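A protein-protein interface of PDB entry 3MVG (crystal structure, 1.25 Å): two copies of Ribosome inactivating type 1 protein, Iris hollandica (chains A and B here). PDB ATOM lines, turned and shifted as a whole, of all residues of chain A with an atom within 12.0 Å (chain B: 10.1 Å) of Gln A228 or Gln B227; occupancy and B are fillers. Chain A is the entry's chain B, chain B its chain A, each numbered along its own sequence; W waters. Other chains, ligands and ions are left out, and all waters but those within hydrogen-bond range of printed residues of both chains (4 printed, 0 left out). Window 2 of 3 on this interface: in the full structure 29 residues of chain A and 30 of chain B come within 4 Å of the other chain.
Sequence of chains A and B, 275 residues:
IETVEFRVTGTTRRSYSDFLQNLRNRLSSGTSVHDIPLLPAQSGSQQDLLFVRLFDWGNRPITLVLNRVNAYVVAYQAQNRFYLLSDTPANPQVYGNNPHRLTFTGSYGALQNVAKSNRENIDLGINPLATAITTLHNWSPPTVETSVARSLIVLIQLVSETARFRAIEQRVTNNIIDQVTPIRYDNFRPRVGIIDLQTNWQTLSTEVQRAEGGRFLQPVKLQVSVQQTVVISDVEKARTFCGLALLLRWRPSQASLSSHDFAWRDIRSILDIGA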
ATOM      1  N   ARG A 191      -6.190 -13.238  12.663  1.00  0.00           N
ATOM      2  CA  ARG A 191      -7.396 -13.621  11.951  1.00  0.00           C
ATOM      3  C   ARG A 191      -8.541 -12.733  12.410  1.00  0.00           C
ATOM      4  O   ARG A 191      -8.319 -11.617  12.894  1.00  0.00           O
ATOM      5  CB  ARG A 191      -7.702 -15.104  12.176  1.00  0.00           C
ATOM      6  CG  ARG A 191      -8.670 -15.710  11.169  1.00  0.00           C
ATOM      7  CD  ARG A 191      -9.031 -17.136  11.552  1.00  0.00           C
ATOM      8  NE  ARG A 191      -7.895 -18.046  11.416  1.00  0.00           N
ATOM      9  CZ  ARG A 191      -7.965 -19.360  11.605  1.00  0.00           C
ATOM     10  NH1 ARG A 191      -9.117 -19.927  11.943  1.00  0.00           N
ATOM     11  NH2 ARG A 191      -6.881 -20.112  11.456  1.00  0.00           N
ATOM     12  N   VAL A 192      -9.777 -13.236  12.244  1.00  0.00           N
ATOM     13  CA  VAL A 192     -10.978 -12.475  12.557  1.00  0.00           C
ATOM     14  C   VAL A 192     -11.011 -11.940  13.999  1.00  0.00           C
ATOM     15  O   VAL A 192     -11.349 -10.777  14.216  1.00  0.00           O
ATOM     16  CB  VAL A 192     -12.258 -13.289  12.182  1.00  0.00           C
ATOM     17  CG1 VAL A 192     -12.393 -14.529  13.035  1.00  0.00           C
ATOM     18  CG2 VAL A 192     -13.503 -12.435  12.268  1.00  0.00           C
ATOM     19  N   GLY A 193     -10.610 -12.769  14.959  1.00  0.00           N
ATOM     20  CA  GLY A 193     -10.627 -12.389  16.366  1.00  0.00           C
ATOM     21  C   GLY A 193      -9.686 -11.250  16.713  1.00  0.00           C
ATOM     22  O   GLY A 193     -10.102 -10.242  17.295  1.00  0.00           O
ATOM     23  N   ILE A 194      -8.416 -11.405  16.355  1.00  0.00           N
ATOM     24  CA  ILE A 194      -7.415 -10.378  16.637  1.00  0.00           C
ATOM     25  C   ILE A 194      -7.741  -9.072  15.919  1.00  0.00           C
ATOM     26  O   ILE A 194      -7.646  -7.997  16.507  1.00  0.00           O
ATOM     27  CB  ILE A 194      -6.001 -10.834  16.247  1.00  0.00           C
ATOM     28  CG1 ILE A 194      -5.513 -11.920  17.205  1.00  0.00           C
ATOM     29  CG2 ILE A 194      -5.047  -9.645  16.247  1.00  0.00           C
ATOM     30  CD1 ILE A 194      -4.248 -12.601  16.740  1.00  0.00           C
ATOM     31  N   ILE A 195      -8.138  -9.172  14.654  1.00  0.00           N
ATOM     32  CA  ILE A 195      -8.485  -7.990  13.869  1.00  0.00           C
ATOM     33  C   ILE A 195      -9.649  -7.227  14.509  1.00  0.00           C
ATOM     34  O   ILE A 195      -9.590  -6.000  14.644  1.00  0.00           O
ATOM     35  CB  ILE A 195      -8.747  -8.361  12.395  1.00  0.00           C
ATOM     36  CG1 ILE A 195      -7.405  -8.686  11.728  1.00  0.00           C
ATOM     37  CG2 ILE A 195      -9.460  -7.225  11.656  1.00  0.00           C
ATOM     38  CD1 ILE A 195      -7.502  -9.368  10.394  1.00  0.00           C
ATOM     39  N   ASP A 196     -10.680  -7.945  14.949  1.00  0.00           N
ATOM     40  CA  ASP A 196     -11.814  -7.273  15.574  1.00  0.00           C
ATOM     41  C   ASP A 196     -11.454  -6.694  16.939  1.00  0.00           C
ATOM     42  O   ASP A 196     -11.980  -5.656  17.342  1.00  0.00           O
ATOM     43  CB  ASP A 196     -13.024  -8.192  15.694  1.00  0.00           C
ATOM     44  CG  ASP A 196     -14.319  -7.417  15.740  1.00  0.00           C
ATOM     45  OD1 ASP A 196     -14.452  -6.439  14.981  1.00  0.00           O
ATOM     46  OD2 ASP A 196     -15.202  -7.784  16.527  1.00  0.00           O
ATOM     47  N   LEU A 197     -10.554  -7.359  17.654  1.00  0.00           N
ATOM     48  CA  LEU A 197     -10.059  -6.823  18.912  1.00  0.00           C
ATOM     49  C   LEU A 197      -9.368  -5.473  18.680  1.00  0.00           C
ATOM     50  O   LEU A 197      -9.661  -4.478  19.350  1.00  0.00           O
ATOM     51  CB  LEU A 197      -9.114  -7.823  19.580  1.00  0.00           C
ATOM     52  CG  LEU A 197      -8.655  -7.473  20.995  1.00  0.00           C
ATOM     53  CD1 LEU A 197      -9.831  -7.389  21.966  1.00  0.00           C
ATOM     54  CD2 LEU A 197      -7.636  -8.494  21.475  1.00  0.00           C
ATOM     55  N   ASN A 200     -11.651  -2.543  18.136  1.00  0.00           N
ATOM     56  CA  ASN A 200     -12.485  -2.189  19.283  1.00  0.00           C
ATOM     57  C   ASN A 200     -11.760  -1.592  20.482  1.00  0.00           C
ATOM     58  O   ASN A 200     -12.342  -1.473  21.557  1.00  0.00           O
ATOM     59  CB  ASN A 200     -13.330  -3.394  19.696  1.00  0.00           C
ATOM     60  CG  ASN A 200     -14.557  -3.543  18.834  1.00  0.00           C
ATOM     61  OD1 ASN A 200     -15.526  -2.798  18.991  1.00  0.00           O
ATOM     62  ND2 ASN A 200     -14.510  -4.474  17.889  1.00  0.00           N
ATOM     63  N   VAL A 220     -19.750  -4.730  24.581  1.00  0.00           N
ATOM     64  CA  VAL A 220     -19.003  -4.736  23.326  1.00  0.00           C
ATOM     65  C   VAL A 220     -18.983  -6.134  22.701  1.00  0.00           C
ATOM     66  O   VAL A 220     -18.500  -7.087  23.313  1.00  0.00           O
ATOM     67  CB  VAL A 220     -17.552  -4.259  23.569  1.00  0.00           C
ATOM     68  CG1 VAL A 220     -16.777  -4.187  22.261  1.00  0.00           C
ATOM     69  CG2 VAL A 220     -17.541  -2.904  24.278  1.00  0.00           C
ATOM     70  N   LYS A 221     -19.517  -6.251  21.484  1.00  0.00           N
ATOM     71  CA  LYS A 221     -19.474  -7.510  20.735  1.00  0.00           C
ATOM     72  C   LYS A 221     -18.131  -7.652  20.031  1.00  0.00           C
ATOM     73  O   LYS A 221     -17.674  -6.710  19.381  1.00  0.00           O
ATOM     74  CB  LYS A 221     -20.612  -7.579  19.716  1.00  0.00           C
ATOM     75  CG  LYS A 221     -21.995  -7.685  20.345  1.00  0.00           C
ATOM     76  CD  LYS A 221     -23.121  -7.384  19.354  1.00  0.00           C
ATOM     77  CE  LYS A 221     -23.334  -8.503  18.342  1.00  0.00           C
ATOM     78  NZ  LYS A 221     -24.528  -8.253  17.481  1.00  0.00           N
ATOM     79  N   LEU A 222     -17.502  -8.815  20.189  1.00  0.00           N
ATOM     80  CA  LEU A 222     -16.235  -9.111  19.524  1.00  0.00           C
ATOM     81  C   LEU A 222     -16.342 -10.394  18.724  1.00  0.00           C
ATOM     82  O   LEU A 222     -16.799 -11.421  19.233  1.00  0.00           O
ATOM     83  CB  LEU A 222     -15.102  -9.269  20.536  1.00  0.00           C
ATOM     84  CG  LEU A 222     -14.685  -8.054  21.362  1.00  0.00           C
ATOM     85  CD1 LEU A 222     -13.599  -8.454  22.335  1.00  0.00           C
ATOM     86  CD2 LEU A 222     -14.197  -6.919  20.477  1.00  0.00           C
ATOM     87  N   GLN A 223     -15.911 -10.333  17.469  1.00  0.00           N
ATOM     88  CA  GLN A 223     -15.908 -11.512  16.611  1.00  0.00           C
ATOM     89  C   GLN A 223     -14.930 -12.550  17.145  1.00  0.00           C
ATOM     90  O   GLN A 223     -13.811 -12.225  17.547  1.00  0.00           O
ATOM     91  CB  GLN A 223     -15.543 -11.138  15.174  1.00  0.00           C
ATOM     92  CG  GLN A 223     -16.564 -10.249  14.483  1.00  0.00           C
ATOM     93  CD  GLN A 223     -17.838 -10.988  14.105  1.00  0.00           C
ATOM     94  OE1 GLN A 223     -17.826 -12.196  13.859  1.00  0.00           O
ATOM     95  NE2 GLN A 223     -18.946 -10.259  14.048  1.00  0.00           N
ATOM     96  N   VAL A 224     -15.370 -13.800  17.175  1.00  0.00           N
ATOM     97  CA  VAL A 224     -14.476 -14.924  17.508  1.00  0.00           C
ATOM     98  C   VAL A 224     -14.303 -15.852  16.303  1.00  0.00           C
ATOM     99  O   VAL A 224     -13.342 -16.611  16.230  1.00  0.00           O
ATOM    100  CB  VAL A 224     -14.938 -15.730  18.751  1.00  0.00           C
ATOM    101  CG1 VAL A 224     -14.851 -14.878  20.008  1.00  0.00           C
ATOM    102  CG2 VAL A 224     -16.353 -16.295  18.558  1.00  0.00           C
ATOM    103  N   SER A 225     -15.256 -15.782  15.377  1.00  0.00           N
ATOM    104  CA  SER A 225     -15.207 -16.495  14.105  1.00  0.00           C
ATOM    105  C   SER A 225     -15.967 -15.633  13.116  1.00  0.00           C
ATOM    106  O   SER A 225     -16.592 -14.652  13.501  1.00  0.00           O
ATOM    107  CB  SER A 225     -15.860 -17.877  14.225  1.00  0.00           C
ATOM    108  OG  SER A 225     -17.269 -17.776  14.372  1.00  0.00           O
ATOM    109  N   VAL A 226     -15.948 -16.007  11.842  1.00  0.00           N
ATOM    110  CA  VAL A 226     -16.742 -15.296  10.846  1.00  0.00           C
ATOM    111  C   VAL A 226     -18.239 -15.302  11.208  1.00  0.00           C
ATOM    112  O   VAL A 226     -18.952 -14.330  10.950  1.00  0.00           O
ATOM    113  CB  VAL A 226     -16.496 -15.878   9.429  1.00  0.00           C
ATOM    114  CG1 VAL A 226     -17.329 -15.160   8.391  1.00  0.00           C
ATOM    115  CG2 VAL A 226     -15.017 -15.775   9.063  1.00  0.00           C
ATOM    116  N   GLN A 227     -18.692 -16.380  11.843  1.00  0.00           N
ATOM    117  CA  GLN A 227     -20.113 -16.580  12.132  1.00  0.00           C
ATOM    118  C   GLN A 227     -20.585 -16.077  13.492  1.00  0.00           C
ATOM    119  O   GLN A 227     -21.782 -15.854  13.682  1.00  0.00           O
ATOM    120  CB  GLN A 227     -20.469 -18.067  12.027  1.00  0.00           C
ATOM    121  CG  GLN A 227     -20.397 -18.632  10.614  1.00  0.00           C
ATOM    122  CD  GLN A 227     -18.975 -18.854  10.138  1.00  0.00           C
ATOM    123  OE1 GLN A 227     -18.092 -19.258  10.908  1.00  0.00           O
ATOM    124  NE2 GLN A 227     -18.743 -18.596   8.857  1.00  0.00           N
ATOM    125  N   GLN A 228     -19.666 -15.924  14.444  1.00  0.00           N
ATOM    126  CA  GLN A 228     -20.073 -15.703  15.827  1.00  0.00           C
ATOM    127  C   GLN A 228     -19.287 -14.651  16.573  1.00  0.00           C
ATOM    128  O   GLN A 228     -18.126 -14.374  16.283  1.00  0.00           O
ATOM    129  CB  GLN A 228     -20.028 -16.998  16.624  1.00  0.00           C
ATOM    130  CG  GLN A 228     -21.066 -18.019  16.204  1.00  0.00           C
ATOM    131  CD  GLN A 228     -21.176 -19.152  17.189  1.00  0.00           C
ATOM    132  OE1 GLN A 228     -20.232 -19.916  17.383  1.00  0.00           O
ATOM    133  NE2 GLN A 228     -22.332 -19.266  17.830  1.00  0.00           N
ATOM    134  N   THR A 229     -19.948 -14.122  17.588  1.00  0.00           N
ATOM    135  CA  THR A 229     -19.482 -12.980  18.318  1.00  0.00           C
ATOM    136  C   THR A 229     -19.655 -13.314  19.804  1.00  0.00           C
ATOM    137  O   THR A 229     -20.618 -13.990  20.177  1.00  0.00           O
ATOM    138  CB  THR A 229     -20.331 -11.770  17.836  1.00  0.00           C
ATOM    139  OG1 THR A 229     -19.501 -10.678  17.422  1.00  0.00           O
ATOM    140  CG2 THR A 229     -21.382 -11.352  18.838  1.00  0.00           C
ATOM    141  N   VAL A 230     -18.699 -12.907  20.641  1.00  0.00           N
ATOM    142  CA  VAL A 230     -18.900 -12.921  22.095  1.00  0.00           C
ATOM    143  C   VAL A 230     -19.108 -11.496  22.592  1.00  0.00           C
ATOM    144  O   VAL A 230     -18.800 -10.534  21.894  1.00  0.00           O
ATOM    145  CB  VAL A 230     -17.750 -13.609  22.883  1.00  0.00           C
ATOM    146  CG1 VAL A 230     -17.653 -15.093  22.526  1.00  0.00           C
ATOM    147  CG2 VAL A 230     -16.420 -12.892  22.671  1.00  0.00           C
ATOM    148  N   VAL A 231     -19.649 -11.370  23.797  1.00  0.00           N
ATOM    149  CA  VAL A 231     -19.963 -10.067  24.356  1.00  0.00           C
ATOM    150  C   VAL A 231     -19.097  -9.800  25.585  1.00  0.00           C
ATOM    151  O   VAL A 231     -18.999 -10.638  26.479  1.00  0.00           O
ATOM    152  CB  VAL A 231     -21.472  -9.963  24.701  1.00  0.00           C
ATOM    153  CG1 VAL A 231     -21.815  -8.584  25.233  1.00  0.00           C
ATOM    154  CG2 VAL A 231     -22.330 -10.277  23.471  1.00  0.00           C
ATOM    155  N   ILE A 232     -18.448  -8.637  25.593  1.00  0.00           N
ATOM    156  CA  ILE A 232     -17.680  -8.157  26.741  1.00  0.00           C
ATOM    157  C   ILE A 232     -18.559  -7.148  27.476  1.00  0.00           C
ATOM    158  O   ILE A 232     -18.869  -6.085  26.939  1.00  0.00           O
ATOM    159  CB  ILE A 232     -16.345  -7.493  26.303  1.00  0.00           C
ATOM    160  CG1 ILE A 232     -15.581  -8.355  25.277  1.00  0.00           C
ATOM    161  CG2 ILE A 232     -15.489  -7.134  27.524  1.00  0.00           C
ATOM    162  CD1 ILE A 232     -15.319  -9.804  25.681  1.00  0.00           C
ATOM    163  N   LYS A 237     -13.893  -8.879  32.485  1.00  0.00           N
ATOM    164  CA  LYS A 237     -13.759  -9.575  31.219  1.00  0.00           C
ATOM    165  C   LYS A 237     -12.798  -8.839  30.279  1.00  0.00           C
ATOM    166  O   LYS A 237     -11.986  -9.465  29.598  1.00  0.00           O
ATOM    167  CB  LYS A 237     -15.128  -9.760  30.571  1.00  0.00           C
ATOM    168  CG  LYS A 237     -15.126 -10.649  29.336  1.00  0.00           C
ATOM    169  CD  LYS A 237     -15.312 -12.121  29.657  1.00  0.00           C
ATOM    170  CE  LYS A 237     -15.529 -12.917  28.375  1.00  0.00           C
ATOM    171  NZ  LYS A 237     -15.893 -14.338  28.633  1.00  0.00           N
ATOM    172  N   PHE A 241     -10.004 -11.438  29.670  1.00  0.00           N
ATOM    173  CA  PHE A 241     -10.169 -12.084  28.364  1.00  0.00           C
ATOM    174  C   PHE A 241      -9.435 -11.324  27.245  1.00  0.00           C
ATOM    175  O   PHE A 241      -8.673 -11.915  26.474  1.00  0.00           O
ATOM    176  CB  PHE A 241     -11.664 -12.239  28.044  1.00  0.00           C
ATOM    177  CG  PHE A 241     -11.945 -12.884  26.717  1.00  0.00           C
ATOM    178  CD1 PHE A 241     -11.874 -14.266  26.572  1.00  0.00           C
ATOM    179  CD2 PHE A 241     -12.299 -12.114  25.616  1.00  0.00           C
ATOM    180  CE1 PHE A 241     -12.132 -14.872  25.342  1.00  0.00           C
ATOM    181  CE2 PHE A 241     -12.563 -12.710  24.381  1.00  0.00           C
ATOM    182  CZ  PHE A 241     -12.483 -14.094  24.249  1.00  0.00           C
ATOM    183  N   VAL B 192     -16.562 -20.977  30.738  1.00  0.00           N
ATOM    184  CA  VAL B 192     -16.863 -22.196  29.986  1.00  0.00           C
ATOM    185  C   VAL B 192     -15.735 -22.500  28.982  1.00  0.00           C
ATOM    186  O   VAL B 192     -15.401 -23.664  28.723  1.00  0.00           O
ATOM    187  CB  VAL B 192     -18.250 -22.068  29.289  1.00  0.00           C
ATOM    188  CG1 VAL B 192     -18.438 -23.107  28.195  1.00  0.00           C
ATOM    189  CG2 VAL B 192     -19.368 -22.160  30.329  1.00  0.00           C
ATOM    190  N   GLY B 193     -15.146 -21.436  28.442  1.00  0.00           N
ATOM    191  CA  GLY B 193     -14.025 -21.538  27.518  1.00  0.00           C
ATOM    192  C   GLY B 193     -12.794 -22.153  28.155  1.00  0.00           C
ATOM    193  O   GLY B 193     -12.173 -23.039  27.578  1.00  0.00           O
ATOM    194  N   LYS B 221     -13.142 -28.926  18.099  1.00  0.00           N
ATOM    195  CA  LYS B 221     -14.059 -27.845  18.436  1.00  0.00           C
ATOM    196  C   LYS B 221     -13.935 -27.498  19.917  1.00  0.00           C
ATOM    197  O   LYS B 221     -13.938 -28.382  20.773  1.00  0.00           O
ATOM    198  CB  LYS B 221     -15.498 -28.231  18.100  1.00  0.00           C
ATOM    199  CG  LYS B 221     -16.504 -27.109  18.332  1.00  0.00           C
ATOM    200  CD  LYS B 221     -17.944 -27.563  18.096  1.00  0.00           C
ATOM    201  CE  LYS B 221     -18.407 -28.567  19.146  1.00  0.00           C
ATOM    202  NZ  LYS B 221     -18.797 -27.939  20.428  1.00  0.00           N
ATOM    203  N   LEU B 222     -13.831 -26.202  20.196  1.00  0.00           N
ATOM    204  CA  LEU B 222     -13.740 -25.695  21.564  1.00  0.00           C
ATOM    205  C   LEU B 222     -14.806 -24.650  21.828  1.00  0.00           C
ATOM    206  O   LEU B 222     -15.056 -23.784  20.993  1.00  0.00           O
ATOM    207  CB  LEU B 222     -12.370 -25.060  21.821  1.00  0.00           C
ATOM    208  CG  LEU B 222     -11.122 -25.940  21.775  1.00  0.00           C
ATOM    209  CD1 LEU B 222      -9.890 -25.066  21.935  1.00  0.00           C
ATOM    210  CD2 LEU B 222     -11.152 -27.013  22.849  1.00  0.00           C
ATOM    211  N   GLN B 223     -15.420 -24.727  23.001  1.00  0.00           N
ATOM    212  CA  GLN B 223     -16.293 -23.657  23.462  1.00  0.00           C
ATOM    213  C   GLN B 223     -15.465 -22.442  23.832  1.00  0.00           C
ATOM    214  O   GLN B 223     -14.423 -22.570  24.480  1.00  0.00           O
ATOM    215  CB  GLN B 223     -17.080 -24.093  24.697  1.00  0.00           C
ATOM    216  CG  GLN B 223     -17.937 -25.322  24.492  1.00  0.00           C
ATOM    217  CD  GLN B 223     -19.106 -25.105  23.544  1.00  0.00           C
ATOM    218  OE1 GLN B 223     -19.709 -24.026  23.496  1.00  0.00           O
ATOM    219  NE2 GLN B 223     -19.439 -26.140  22.792  1.00  0.00           N
ATOM    220  N   VAL B 224     -15.915 -21.263  23.420  1.00  0.00           N
ATOM    221  CA  VAL B 224     -15.360 -20.025  23.963  1.00  0.00           C
ATOM    222  C   VAL B 224     -16.354 -19.395  24.939  1.00  0.00           C
ATOM    223  O   VAL B 224     -15.998 -18.509  25.712  1.00  0.00           O
ATOM    224  CB  VAL B 224     -14.908 -19.025  22.868  1.00  0.00           C
ATOM    225  CG1 VAL B 224     -13.761 -19.616  22.053  1.00  0.00           C
ATOM    226  CG2 VAL B 224     -16.060 -18.621  21.965  1.00  0.00           C
ATOM    227  N   SER B 225     -17.596 -19.874  24.883  1.00  0.00           N
ATOM    228  CA  SER B 225     -18.686 -19.467  25.768  1.00  0.00           C
ATOM    229  C   SER B 225     -19.737 -20.569  25.695  1.00  0.00           C
ATOM    230  O   SER B 225     -19.534 -21.569  25.009  1.00  0.00           O
ATOM    231  CB  SER B 225     -19.285 -18.140  25.305  1.00  0.00           C
ATOM    232  OG  SER B 225     -19.845 -18.280  24.009  1.00  0.00           O
ATOM    233  N   VAL B 226     -20.860 -20.394  26.386  1.00  0.00           N
ATOM    234  CA  VAL B 226     -21.950 -21.370  26.296  1.00  0.00           C
ATOM    235  C   VAL B 226     -22.445 -21.497  24.849  1.00  0.00           C
ATOM    236  O   VAL B 226     -22.664 -22.606  24.356  1.00  0.00           O
ATOM    237  CB  VAL B 226     -23.126 -21.015  27.249  1.00  0.00           C
ATOM    238  CG1 VAL B 226     -24.257 -22.035  27.129  1.00  0.00           C
ATOM    239  CG2 VAL B 226     -22.646 -20.936  28.693  1.00  0.00           C
ATOM    240  N   GLN B 227     -22.577 -20.359  24.173  1.00  0.00           N
ATOM    241  CA  GLN B 227     -23.232 -20.291  22.861  1.00  0.00           C
ATOM    242  C   GLN B 227     -22.275 -20.243  21.668  1.00  0.00           C
ATOM    243  O   GLN B 227     -22.692 -20.477  20.531  1.00  0.00           O
ATOM    244  CB  GLN B 227     -24.163 -19.070  22.796  1.00  0.00           C
ATOM    245  CG  GLN B 227     -25.235 -18.985  23.893  1.00  0.00           C
ATOM    246  CD  GLN B 227     -26.356 -19.999  23.735  1.00  0.00           C
ATOM    247  OE1 GLN B 227     -26.552 -20.582  22.664  1.00  0.00           O
ATOM    248  NE2 GLN B 227     -27.109 -20.208  24.810  1.00  0.00           N
ATOM    249  N   GLN B 228     -21.005 -19.924  21.912  1.00  0.00           N
ATOM    250  CA  GLN B 228     -20.055 -19.720  20.814  1.00  0.00           C
ATOM    251  C   GLN B 228     -18.877 -20.681  20.861  1.00  0.00           C
ATOM    252  O   GLN B 228     -18.403 -21.061  21.941  1.00  0.00           O
ATOM    253  CB  GLN B 228     -19.565 -18.269  20.774  1.00  0.00           C
ATOM    254  CG  GLN B 228     -20.618 -17.261  20.307  1.00  0.00           C
ATOM    255  CD  GLN B 228     -21.520 -16.747  21.423  1.00  0.00           C
ATOM    256  OE1 GLN B 228     -21.083 -16.547  22.560  1.00  0.00           O
ATOM    257  NE2 GLN B 228     -22.783 -16.498  21.086  1.00  0.00           N
ATOM    258  N   THR B 229     -18.410 -21.059  19.674  1.00  0.00           N
ATOM    259  CA  THR B 229     -17.341 -22.035  19.517  1.00  0.00           C
ATOM    260  C   THR B 229     -16.312 -21.573  18.498  1.00  0.00           C
ATOM    261  O   THR B 229     -16.574 -20.687  17.675  1.00  0.00           O
ATOM    262  CB  THR B 229     -17.891 -23.393  19.033  1.00  0.00           C
ATOM    263  OG1 THR B 229     -18.707 -23.191  17.872  1.00  0.00           O
ATOM    264  CG2 THR B 229     -18.704 -24.084  20.117  1.00  0.00           C
ATOM    265  N   VAL B 230     -15.125 -22.170  18.579  1.00  0.00           N
ATOM    266  CA  VAL B 230     -14.127 -22.070  17.523  1.00  0.00           C
ATOM    267  C   VAL B 230     -13.621 -23.482  17.211  1.00  0.00           C
ATOM    268  O   VAL B 230     -13.859 -24.427  17.969  1.00  0.00           O
ATOM    269  CB  VAL B 230     -12.947 -21.141  17.913  1.00  0.00           C
ATOM    270  CG1 VAL B 230     -13.424 -19.714  18.193  1.00  0.00           C
ATOM    271  CG2 VAL B 230     -12.163 -21.711  19.099  1.00  0.00           C
ATOM    272  N   VAL B 231     -12.922 -23.624  16.093  1.00  0.00           N
ATOM    273  CA  VAL B 231     -12.363 -24.914  15.718  1.00  0.00           C
ATOM    274  C   VAL B 231     -10.857 -24.770  15.544  1.00  0.00           C
ATOM    275  O   VAL B 231     -10.383 -23.864  14.854  1.00  0.00           O
ATOM    276  CB  VAL B 231     -13.009 -25.469  14.427  1.00  0.00           C
ATOM    277  CG1 VAL B 231     -12.366 -26.800  14.029  1.00  0.00           C
ATOM    278  CG2 VAL B 231     -14.524 -25.620  14.605  1.00  0.00           C
HETATM  279  O   HOH W   1     -18.202 -19.934  15.641  1.00  0.00           O
HETATM  280  O   HOH W   2     -21.515 -22.705  18.413  1.00  0.00           O
HETATM  281  O   HOH W   3     -23.363 -13.127  20.548  1.00  0.00           O
HETATM  282  O   HOH W   4     -21.149 -13.902  24.604  1.00  0.00           O
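Val A224 touches Val B230 (O to CG1, 3.7 Å). Gln A228 touches Gln B228. Val B224 touches Val A230 (CG2 to CG1, 3.9 Å). Gln B228 touches Val A230 (OE1 to CG1, 3.7 Å).
Water W1 lies within hydrogen-bond range of OG of Ser A225 (2.7 Å), OE1 of Gln A228 (2.7 Å) and O of Thr B229 (2.7 Å). Water W2 lies within hydrogen-bond range of OG1 of Thr B229, OE1 of Gln A228 and O of Gln B227. Water W3 bridges the backbone carbonyl oxygen (O) of Thr A229 (2.9 Å) and the side-chain amide nitrogen (NE2) of Gln B228 (3.5 Å). Water W4 bridges N of Val A231 and OE1 of Gln B228.
Val A224 touches Val B230, and with the chains exchanged Val A230 touches Val B224. Gln A228 touches Gln B227, but with the chains exchanged Gln A227 does not touch Gln B228 (6.9 Å). Gln A228 touches its own counterpart, Gln B228. Val A230 touches Gln B228, but with the chains exchanged Gln A228 does not touch Val B230 (5.7 Å). Of the 7 pairs that touch across the chains among the printed residues, 5 have their exchanged pair printed and touching as well.
Of chain B, only Gln B227 (3.0 Å), Gln B228 (3.4 Å) and Thr B229 (3.1 Å) come within 4 Å of Gln A228. Gln B227 touches just one residue of chain A: Gln A228. Val A224 touches just one residue of chain B: Val B230. No residue of chain B comes within 4 Å of Ser A225. No residue of chain A comes within 4 Å of Ser B225. No residue of chain A comes within 4 Å of Val B226. Gln B228 touches just these residues of chain A: Gln A228 (3.4 Å), Thr A229 (3.2 Å) and Val A230 (3.7 Å). Of the printed residues of chain B, Val A230 touches Val B224 (3.9 Å) and Gln B228 (3.7 Å). Of the printed residues of chain A, Val B230 touches Val A224 (3.7 Å). Of the printed residues of chain A, Val B224 touches Val A230 (3.9 Å). The nearest residue of chain A that does not touch Gln B227 is Thr A229 (6.6 Å). The nearest printed residue of chain B that does not touch Val A230 is Ser B225 (4.1 Å).
The backbone carbonyl oxygen (O) of Gln B227 is in hydrogen-bond range of the side-chain amide nitrogen (NE2) of Gln A228, 3.0 Å away. OE1 of Gln A228 sits at hydrogen-bond distance from N of Thr B229. O of Thr A229 sits close to NE2 of Gln B228, at 3.4 Å.
Of the 23 printed residues of chain A, 4 touch a printed residue of chain B. Hydrophobic or aromatic side chains of chain A within 4 Å of the printed part of chain B: Val A230.
The backbone NH (N) of Gln A228 is in hydrogen-bond range of the side-chain hydroxyl (OG) of Ser A225. The side-chain amide oxygen (OE1) of Gln B228 sits at hydrogen-bond distance from the side-chain hydroxyl (OG) of Ser B225, at 2.6 Å. The side-chain amide oxygen (OE1) of Gln A223 sits close to the backbone carbonyl oxygen (O) of Gln A228 (3.3 Å). OG of Ser B225 sits close to N of Gln B227 (3.4 Å). The side-chain hydroxyl of Thr A229 lies close to the backbone carbonyl oxygen of Leu A222 (3.3 Å). N of Leu A222 lies within hydrogen-bond range of O of Val A230.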
